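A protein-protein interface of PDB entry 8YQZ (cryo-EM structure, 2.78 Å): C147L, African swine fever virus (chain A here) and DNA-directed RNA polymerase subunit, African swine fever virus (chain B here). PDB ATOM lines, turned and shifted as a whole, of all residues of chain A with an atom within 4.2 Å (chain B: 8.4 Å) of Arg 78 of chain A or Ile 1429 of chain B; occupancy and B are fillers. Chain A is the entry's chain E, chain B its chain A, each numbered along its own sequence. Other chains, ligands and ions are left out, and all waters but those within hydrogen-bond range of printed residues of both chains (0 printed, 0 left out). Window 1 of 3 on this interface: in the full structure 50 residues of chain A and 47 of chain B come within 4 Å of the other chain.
NH1 of Arg 78 of chain A is in hydrogen-bond range of SD of Met 1425 of chain B (3.8 Å).
OG of Ser 1427 of chain B is in hydrogen-bond range of OE2 of Glu 75 of chain A (3.0 Å).
The backbone NH (N) of Leu 118 of chain A is in hydrogen-bond range of the backbone carbonyl oxygen (O) of Ile 1430 of chain B, 2.8 Å away.
Among the printed residues, merely in contact across the chains: Phe 74 of chain A with Leu 480 of chain B, Phe 74 of chain A with Gly 1423 of chain B, Phe 74 of chain A with Thr 1424 of chain B, Thr 77 of chain A with Val 475 of chain B, Thr 77 of chain A with Glu 476 of chain B, Thr 77 of chain A with Leu 479 of chain B, Thr 77 of chain A with Leu 480 of chain B, Thr 77 of chain A with Thr 1424 of chain B, Arg 78 of chain A with Thr 1424 of chain B, Arg 78 of chain A with Ile 1429 of chain B, Val 80 of chain A with Val 475 of chain B, Ala 81 of chain A with Met 472 of chain B, Ala 81 of chain A with Val 475 of chain B, Leu 117 of chain A with Ile 1430 of chain B, Leu 117 of chain A with Met 1431 of chain B, Leu 117 of chain A with Asp 1432 of chain B, Leu 118 of chain A with Ile 1429 of chain B and Leu 118 of chain A with Asp 1432 of chain B.
Of chain B, only Thr 1424 (3.5 Å), Met 1425 (3.8 Å) and Ile 1429 (3.7 Å) come within 4 Å of Arg 78 of chain A.
Of the printed residues of chain B, Val 80 of chain A touches Val 475.
Of the printed residues of chain A, Glu 476 of chain B touches Thr 77.
Of the printed residues of chain A, Thr 1424 of chain B touches Phe 74, Thr 77 and Arg 78.
The nearest residue of chain B that does not touch Arg 78 of chain A is Met 472 of chain B (4.1 Å).
Printed residues of chain A that touch a printed residue of chain B: Phe 74, Glu 75, Thr 77, Arg 78, Val 80, Ala 81, Leu 117 and Leu 118.
Printed residues of chain B that touch a printed residue of chain A: Met 472, Val 475, Glu 476, Leu 479, Leu 480, Gly 1423, Thr 1424, Met 1425, Ser 1427, Ile 1429, Ile 1430, Met 1431 and Asp 1432.
Hydrophobic or aromatic side chains of chain B within 4 Å of the printed part of chain A: Met 472, Val 475, Leu 479, Leu 480, Met 1425, Ile 1429, Ile 1430 and Met 1431.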
ATOM      1  N   PHE A  74      24.636  10.419 -26.909  1.00  0.00           N
ATOM      2  CA  PHE A  74      24.119  11.589 -26.204  1.00  0.00           C
ATOM      3  C   PHE A  74      23.407  11.208 -24.908  1.00  0.00           C
ATOM      4  O   PHE A  74      23.602  11.850 -23.874  1.00  0.00           O
ATOM      5  CB  PHE A  74      23.150  12.345 -27.106  1.00  0.00           C
ATOM      6  CG  PHE A  74      23.758  12.941 -28.338  1.00  0.00           C
ATOM      7  CD1 PHE A  74      25.023  13.479 -28.323  1.00  0.00           C
ATOM      8  CD2 PHE A  74      23.020  13.020 -29.507  1.00  0.00           C
ATOM      9  CE1 PHE A  74      25.546  14.052 -29.450  1.00  0.00           C
ATOM     10  CE2 PHE A  74      23.547  13.591 -30.631  1.00  0.00           C
ATOM     11  CZ  PHE A  74      24.811  14.109 -30.598  1.00  0.00           C
ATOM     12  N   GLU A  75      22.556  10.184 -24.951  1.00  0.00           N
ATOM     13  CA  GLU A  75      21.784   9.805 -23.774  1.00  0.00           C
ATOM     14  C   GLU A  75      22.666   9.199 -22.694  1.00  0.00           C
ATOM     15  O   GLU A  75      22.492   9.495 -21.511  1.00  0.00           O
ATOM     16  CB  GLU A  75      20.675   8.832 -24.168  1.00  0.00           C
ATOM     17  CG  GLU A  75      19.499   9.492 -24.834  1.00  0.00           C
ATOM     18  CD  GLU A  75      18.674   8.550 -25.686  1.00  0.00           C
ATOM     19  OE1 GLU A  75      19.062   7.385 -25.852  1.00  0.00           O
ATOM     20  OE2 GLU A  75      17.638   8.989 -26.212  1.00  0.00           O
ATOM     21  N   ALA A  76      23.618   8.351 -23.077  1.00  0.00           N
ATOM     22  CA  ALA A  76      24.557   7.805 -22.108  1.00  0.00           C
ATOM     23  C   ALA A  76      25.421   8.897 -21.490  1.00  0.00           C
ATOM     24  O   ALA A  76      25.672   8.887 -20.278  1.00  0.00           O
ATOM     25  CB  ALA A  76      25.417   6.741 -22.772  1.00  0.00           C
ATOM     26  N   THR A  77      25.889   9.845 -22.301  1.00  0.00           N
ATOM     27  CA  THR A  77      26.678  10.951 -21.774  1.00  0.00           C
ATOM     28  C   THR A  77      25.876  11.776 -20.779  1.00  0.00           C
ATOM     29  O   THR A  77      26.380  12.125 -19.709  1.00  0.00           O
ATOM     30  CB  THR A  77      27.179  11.823 -22.923  1.00  0.00           C
ATOM     31  OG1 THR A  77      27.827  11.000 -23.892  1.00  0.00           O
ATOM     32  CG2 THR A  77      28.159  12.854 -22.446  1.00  0.00           C
ATOM     33  N   ARG A  78      24.627  12.094 -21.110  1.00  0.00           N
ATOM     34  CA  ARG A  78      23.789  12.865 -20.200  1.00  0.00           C
ATOM     35  C   ARG A  78      23.489  12.097 -18.918  1.00  0.00           C
ATOM     36  O   ARG A  78      23.473  12.685 -17.832  1.00  0.00           O
ATOM     37  CB  ARG A  78      22.503  13.264 -20.910  1.00  0.00           C
ATOM     38  CG  ARG A  78      21.476  13.939 -20.049  1.00  0.00           C
ATOM     39  CD  ARG A  78      21.841  15.365 -19.734  1.00  0.00           C
ATOM     40  NE  ARG A  78      20.745  16.027 -19.042  1.00  0.00           N
ATOM     41  CZ  ARG A  78      20.824  17.206 -18.442  1.00  0.00           C
ATOM     42  NH1 ARG A  78      21.947  17.897 -18.421  1.00  0.00           N
ATOM     43  NH2 ARG A  78      19.750  17.696 -17.836  1.00  0.00           N
ATOM     44  N   LEU A  79      23.240  10.790 -19.015  1.00  0.00           N
ATOM     45  CA  LEU A  79      23.008   9.987 -17.817  1.00  0.00           C
ATOM     46  C   LEU A  79      24.205  10.033 -16.883  1.00  0.00           C
ATOM     47  O   LEU A  79      24.060  10.277 -15.679  1.00  0.00           O
ATOM     48  CB  LEU A  79      22.703   8.540 -18.196  1.00  0.00           C
ATOM     49  CG  LEU A  79      21.325   8.124 -18.692  1.00  0.00           C
ATOM     50  CD1 LEU A  79      21.453   6.802 -19.388  1.00  0.00           C
ATOM     51  CD2 LEU A  79      20.357   8.022 -17.555  1.00  0.00           C
ATOM     52  N   VAL A  80      25.404   9.808 -17.421  1.00  0.00           N
ATOM     53  CA  VAL A  80      26.603   9.821 -16.591  1.00  0.00           C
ATOM     54  C   VAL A  80      26.838  11.206 -15.996  1.00  0.00           C
ATOM     55  O   VAL A  80      27.206  11.328 -14.828  1.00  0.00           O
ATOM     56  CB  VAL A  80      27.814   9.318 -17.396  1.00  0.00           C
ATOM     57  CG1 VAL A  80      29.085   9.534 -16.637  1.00  0.00           C
ATOM     58  CG2 VAL A  80      27.664   7.855 -17.705  1.00  0.00           C
ATOM     59  N   ALA A  81      26.631  12.269 -16.773  1.00  0.00           N
ATOM     60  CA  ALA A  81      26.868  13.616 -16.261  1.00  0.00           C
ATOM     61  C   ALA A  81      25.910  13.972 -15.130  1.00  0.00           C
ATOM     62  O   ALA A  81      26.322  14.518 -14.095  1.00  0.00           O
ATOM     63  CB  ALA A  81      26.756  14.627 -17.396  1.00  0.00           C
ATOM     64  N   VAL A  82      24.622  13.669 -15.306  1.00  0.00           N
ATOM     65  CA  VAL A  82      23.638  13.955 -14.267  1.00  0.00           C
ATOM     66  C   VAL A  82      23.966  13.171 -13.008  1.00  0.00           C
ATOM     67  O   VAL A  82      23.954  13.713 -11.897  1.00  0.00           O
ATOM     68  CB  VAL A  82      22.215  13.651 -14.777  1.00  0.00           C
ATOM     69  CG1 VAL A  82      21.223  13.662 -13.648  1.00  0.00           C
ATOM     70  CG2 VAL A  82      21.807  14.651 -15.821  1.00  0.00           C
ATOM     71  N   LEU A 117      18.217   6.238 -12.752  1.00  0.00           N
ATOM     72  CA  LEU A 117      17.611   7.262 -13.584  1.00  0.00           C
ATOM     73  C   LEU A 117      16.832   6.596 -14.706  1.00  0.00           C
ATOM     74  O   LEU A 117      17.014   5.414 -14.992  1.00  0.00           O
ATOM     75  CB  LEU A 117      18.670   8.215 -14.149  1.00  0.00           C
ATOM     76  CG  LEU A 117      19.494   9.034 -13.154  1.00  0.00           C
ATOM     77  CD1 LEU A 117      20.657   9.701 -13.834  1.00  0.00           C
ATOM     78  CD2 LEU A 117      18.627  10.065 -12.489  1.00  0.00           C
ATOM     79  N   LEU A 118      15.944   7.363 -15.329  1.00  0.00           N
ATOM     80  CA  LEU A 118      15.162   6.897 -16.462  1.00  0.00           C
ATOM     81  C   LEU A 118      15.271   7.897 -17.606  1.00  0.00           C
ATOM     82  O   LEU A 118      15.554   9.073 -17.393  1.00  0.00           O
ATOM     83  CB  LEU A 118      13.695   6.694 -16.085  1.00  0.00           C
ATOM     84  CG  LEU A 118      13.348   5.682 -14.998  1.00  0.00           C
ATOM     85  CD1 LEU A 118      11.903   5.830 -14.632  1.00  0.00           C
ATOM     86  CD2 LEU A 118      13.637   4.276 -15.444  1.00  0.00           C
ATOM     87  N   TYR B   5      11.132  26.341 -11.348  1.00  0.00           N
ATOM     88  CA  TYR B   5      11.891  26.276 -12.589  1.00  0.00           C
ATOM     89  C   TYR B   5      10.959  26.259 -13.793  1.00  0.00           C
ATOM     90  O   TYR B   5       9.971  25.521 -13.814  1.00  0.00           O
ATOM     91  CB  TYR B   5      12.766  25.026 -12.574  1.00  0.00           C
ATOM     92  CG  TYR B   5      13.482  24.714 -13.859  1.00  0.00           C
ATOM     93  CD1 TYR B   5      14.731  25.229 -14.122  1.00  0.00           C
ATOM     94  CD2 TYR B   5      12.906  23.897 -14.808  1.00  0.00           C
ATOM     95  CE1 TYR B   5      15.378  24.936 -15.292  1.00  0.00           C
ATOM     96  CE2 TYR B   5      13.541  23.609 -15.969  1.00  0.00           C
ATOM     97  CZ  TYR B   5      14.776  24.122 -16.205  1.00  0.00           C
ATOM     98  OH  TYR B   5      15.406  23.821 -17.377  1.00  0.00           O
ATOM     99  N   GLU B   7      10.721  27.069 -18.395  1.00  0.00           N
ATOM    100  CA  GLU B   7      11.360  27.296 -19.684  1.00  0.00           C
ATOM    101  C   GLU B   7      10.418  28.067 -20.590  1.00  0.00           C
ATOM    102  O   GLU B   7       9.202  27.909 -20.501  1.00  0.00           O
ATOM    103  CB  GLU B   7      11.752  25.986 -20.364  1.00  0.00           C
ATOM    104  CG  GLU B   7      13.023  25.365 -19.849  1.00  0.00           C
ATOM    105  CD  GLU B   7      12.972  23.858 -19.860  1.00  0.00           C
ATOM    106  OE1 GLU B   7      11.857  23.304 -19.851  1.00  0.00           O
ATOM    107  OE2 GLU B   7      14.042  23.221 -19.870  1.00  0.00           O
ATOM    108  N   MET B 472      29.706  18.254 -14.906  1.00  0.00           N
ATOM    109  CA  MET B 472      28.905  17.955 -16.086  1.00  0.00           C
ATOM    110  C   MET B 472      29.653  18.271 -17.370  1.00  0.00           C
ATOM    111  O   MET B 472      29.525  17.548 -18.360  1.00  0.00           O
ATOM    112  CB  MET B 472      27.591  18.725 -16.038  1.00  0.00           C
ATOM    113  CG  MET B 472      26.549  18.084 -15.177  1.00  0.00           C
ATOM    114  SD  MET B 472      24.900  18.520 -15.705  1.00  0.00           S
ATOM    115  CE  MET B 472      23.959  18.008 -14.300  1.00  0.00           C
ATOM    116  N   VAL B 475      32.429  15.486 -17.777  1.00  0.00           N
ATOM    117  CA  VAL B 475      31.969  14.178 -18.222  1.00  0.00           C
ATOM    118  C   VAL B 475      31.792  14.165 -19.730  1.00  0.00           C
ATOM    119  O   VAL B 475      32.249  13.251 -20.421  1.00  0.00           O
ATOM    120  CB  VAL B 475      30.660  13.799 -17.512  1.00  0.00           C
ATOM    121  CG1 VAL B 475      29.948  12.733 -18.295  1.00  0.00           C
ATOM    122  CG2 VAL B 475      30.928  13.329 -16.116  1.00  0.00           C
ATOM    123  N   GLU B 476      31.138  15.184 -20.268  1.00  0.00           N
ATOM    124  CA  GLU B 476      30.854  15.180 -21.686  1.00  0.00           C
ATOM    125  C   GLU B 476      32.059  15.548 -22.530  1.00  0.00           C
ATOM    126  O   GLU B 476      32.081  15.226 -23.714  1.00  0.00           O
ATOM    127  CB  GLU B 476      29.690  16.109 -21.979  1.00  0.00           C
ATOM    128  CG  GLU B 476      30.084  17.503 -22.185  1.00  0.00           C
ATOM    129  CD  GLU B 476      29.070  18.245 -22.982  1.00  0.00           C
ATOM    130  OE1 GLU B 476      28.057  17.644 -23.358  1.00  0.00           O
ATOM    131  OE2 GLU B 476      29.291  19.432 -23.237  1.00  0.00           O
ATOM    132  N   LEU B 479      33.561  11.847 -22.761  1.00  0.00           N
ATOM    133  CA  LEU B 479      32.772  10.815 -23.428  1.00  0.00           C
ATOM    134  C   LEU B 479      32.327  11.215 -24.825  1.00  0.00           C
ATOM    135  O   LEU B 479      32.157  10.351 -25.687  1.00  0.00           O
ATOM    136  CB  LEU B 479      31.542  10.459 -22.598  1.00  0.00           C
ATOM    137  CG  LEU B 479      31.731   9.795 -21.239  1.00  0.00           C
ATOM    138  CD1 LEU B 479      30.401   9.332 -20.724  1.00  0.00           C
ATOM    139  CD2 LEU B 479      32.704   8.662 -21.336  1.00  0.00           C
ATOM    140  N   LEU B 480      32.137  12.504 -25.071  1.00  0.00           N
ATOM    141  CA  LEU B 480      31.600  12.993 -26.331  1.00  0.00           C
ATOM    142  C   LEU B 480      32.629  13.637 -27.246  1.00  0.00           C
ATOM    143  O   LEU B 480      32.572  13.445 -28.458  1.00  0.00           O
ATOM    144  CB  LEU B 480      30.485  14.002 -26.064  1.00  0.00           C
ATOM    145  CG  LEU B 480      29.365  14.095 -27.083  1.00  0.00           C
ATOM    146  CD1 LEU B 480      28.492  12.881 -27.060  1.00  0.00           C
ATOM    147  CD2 LEU B 480      28.596  15.356 -26.813  1.00  0.00           C
ATOM    148  N   ARG B1421      17.697  22.541 -27.457  1.00  0.00           N
ATOM    149  CA  ARG B1421      17.291  21.204 -27.026  1.00  0.00           C
ATOM    150  C   ARG B1421      17.782  20.193 -28.045  1.00  0.00           C
ATOM    151  O   ARG B1421      17.034  19.718 -28.890  1.00  0.00           O
ATOM    152  CB  ARG B1421      15.785  21.126 -26.871  1.00  0.00           C
ATOM    153  CG  ARG B1421      15.317  19.904 -26.148  1.00  0.00           C
ATOM    154  CD  ARG B1421      13.816  19.794 -26.188  1.00  0.00           C
ATOM    155  NE  ARG B1421      13.185  20.851 -25.407  1.00  0.00           N
ATOM    156  CZ  ARG B1421      13.054  20.834 -24.089  1.00  0.00           C
ATOM    157  NH1 ARG B1421      13.502  19.825 -23.365  1.00  0.00           N
ATOM    158  NH2 ARG B1421      12.459  21.856 -23.485  1.00  0.00           N
ATOM    159  N   GLY B1423      21.397  17.406 -28.986  1.00  0.00           N
ATOM    160  CA  GLY B1423      22.568  16.715 -28.501  1.00  0.00           C
ATOM    161  C   GLY B1423      22.344  16.002 -27.192  1.00  0.00           C
ATOM    162  O   GLY B1423      21.440  15.176 -27.086  1.00  0.00           O
ATOM    163  N   THR B1424      23.168  16.300 -26.189  1.00  0.00           N
ATOM    164  CA  THR B1424      22.984  15.688 -24.879  1.00  0.00           C
ATOM    165  C   THR B1424      21.720  16.184 -24.203  1.00  0.00           C
ATOM    166  O   THR B1424      21.259  15.564 -23.248  1.00  0.00           O
ATOM    167  CB  THR B1424      24.198  15.942 -23.978  1.00  0.00           C
ATOM    168  OG1 THR B1424      24.608  17.306 -24.076  1.00  0.00           O
ATOM    169  CG2 THR B1424      25.354  15.052 -24.370  1.00  0.00           C
ATOM    170  N   MET B1425      21.130  17.258 -24.709  1.00  0.00           N
ATOM    171  CA  MET B1425      19.938  17.850 -24.132  1.00  0.00           C
ATOM    172  C   MET B1425      18.672  17.500 -24.889  1.00  0.00           C
ATOM    173  O   MET B1425      17.645  18.140 -24.680  1.00  0.00           O
ATOM    174  CB  MET B1425      20.105  19.361 -24.046  1.00  0.00           C
ATOM    175  CG  MET B1425      19.838  19.855 -22.662  1.00  0.00           C
ATOM    176  SD  MET B1425      21.229  19.845 -21.550  1.00  0.00           S
ATOM    177  CE  MET B1425      22.003  21.356 -22.041  1.00  0.00           C
ATOM    178  N   TYR B1426      18.716  16.491 -25.750  1.00  0.00           N
ATOM    179  CA  TYR B1426      17.554  16.165 -26.559  1.00  0.00           C
ATOM    180  C   TYR B1426      16.524  15.366 -25.775  1.00  0.00           C
ATOM    181  O   TYR B1426      15.321  15.557 -25.956  1.00  0.00           O
ATOM    182  CB  TYR B1426      17.991  15.406 -27.805  1.00  0.00           C
ATOM    183  CG  TYR B1426      16.900  15.243 -28.817  1.00  0.00           C
ATOM    184  CD1 TYR B1426      16.401  16.328 -29.502  1.00  0.00           C
ATOM    185  CD2 TYR B1426      16.360  14.005 -29.078  1.00  0.00           C
ATOM    186  CE1 TYR B1426      15.404  16.179 -30.409  1.00  0.00           C
ATOM    187  CE2 TYR B1426      15.362  13.851 -29.989  1.00  0.00           C
ATOM    188  CZ  TYR B1426      14.885  14.941 -30.650  1.00  0.00           C
ATOM    189  OH  TYR B1426      13.885  14.805 -31.563  1.00  0.00           O
ATOM    190  N   SER B1427      16.967  14.459 -24.921  1.00  0.00           N
ATOM    191  CA  SER B1427      16.075  13.590 -24.173  1.00  0.00           C
ATOM    192  C   SER B1427      16.043  14.001 -22.711  1.00  0.00           C
ATOM    193  O   SER B1427      17.070  14.369 -22.139  1.00  0.00           O
ATOM    194  CB  SER B1427      16.507  12.129 -24.285  1.00  0.00           C
ATOM    195  OG  SER B1427      16.252  11.616 -25.574  1.00  0.00           O
ATOM    196  N   ASP B1428      14.859  13.936 -22.116  1.00  0.00           N
ATOM    197  CA  ASP B1428      14.669  14.245 -20.709  1.00  0.00           C
ATOM    198  C   ASP B1428      15.189  13.115 -19.836  1.00  0.00           C
ATOM    199  O   ASP B1428      15.162  11.948 -20.228  1.00  0.00           O
ATOM    200  CB  ASP B1428      13.192  14.477 -20.409  1.00  0.00           C
ATOM    201  CG  ASP B1428      12.854  15.935 -20.238  1.00  0.00           C
ATOM    202  OD1 ASP B1428      13.682  16.684 -19.686  1.00  0.00           O
ATOM    203  OD2 ASP B1428      11.751  16.339 -20.654  1.00  0.00           O
ATOM    204  N   ILE B1429      15.667  13.471 -18.650  1.00  0.00           N
ATOM    205  CA  ILE B1429      16.041  12.508 -17.622  1.00  0.00           C
ATOM    206  C   ILE B1429      15.104  12.706 -16.440  1.00  0.00           C
ATOM    207  O   ILE B1429      14.819  13.842 -16.052  1.00  0.00           O
ATOM    208  CB  ILE B1429      17.511  12.676 -17.200  1.00  0.00           C
ATOM    209  CG1 ILE B1429      18.450  12.626 -18.410  1.00  0.00           C
ATOM    210  CG2 ILE B1429      17.901  11.631 -16.191  1.00  0.00           C
ATOM    211  CD1 ILE B1429      18.435  11.337 -19.185  1.00  0.00           C
ATOM    212  N   ILE B1430      14.590  11.610 -15.893  1.00  0.00           N
ATOM    213  CA  ILE B1430      13.778  11.648 -14.686  1.00  0.00           C
ATOM    214  C   ILE B1430      14.345  10.646 -13.692  1.00  0.00           C
ATOM    215  O   ILE B1430      15.052   9.709 -14.055  1.00  0.00           O
ATOM    216  CB  ILE B1430      12.288  11.363 -14.959  1.00  0.00           C
ATOM    217  CG1 ILE B1430      12.098   9.946 -15.476  1.00  0.00           C
ATOM    218  CG2 ILE B1430      11.720  12.360 -15.930  1.00  0.00           C
ATOM    219  CD1 ILE B1430      10.675   9.573 -15.676  1.00  0.00           C
ATOM    220  N   MET B1431      14.036  10.860 -12.421  1.00  0.00           N
ATOM    221  CA  MET B1431      14.592  10.032 -11.363  1.00  0.00           C
ATOM    222  C   MET B1431      13.769   8.759 -11.232  1.00  0.00           C
ATOM    223  O   MET B1431      12.540   8.794 -11.333  1.00  0.00           O
ATOM    224  CB  MET B1431      14.630  10.789 -10.038  1.00  0.00           C
ATOM    225  CG  MET B1431      15.352  12.113 -10.131  1.00  0.00           C
ATOM    226  SD  MET B1431      17.119  12.061  -9.821  1.00  0.00           S
ATOM    227  CE  MET B1431      17.245  10.774  -8.611  1.00  0.00           C
ATOM    228  N   ASP B1432      14.451   7.639 -11.031  1.00  0.00           N
ATOM    229  CA  ASP B1432      13.820   6.325 -10.929  1.00  0.00           C
ATOM    230  C   ASP B1432      13.356   6.109  -9.494  1.00  0.00           C
ATOM    231  O   ASP B1432      14.081   5.580  -8.653  1.00  0.00           O
ATOM    232  CB  ASP B1432      14.796   5.250 -11.374  1.00  0.00           C
ATOM    233  CG  ASP B1432      14.123   3.952 -11.703  1.00  0.00           C
ATOM    234  OD1 ASP B1432      12.909   3.817 -11.453  1.00  0.00           O
ATOM    235  OD2 ASP B1432      14.815   3.052 -12.212  1.00  0.00           O
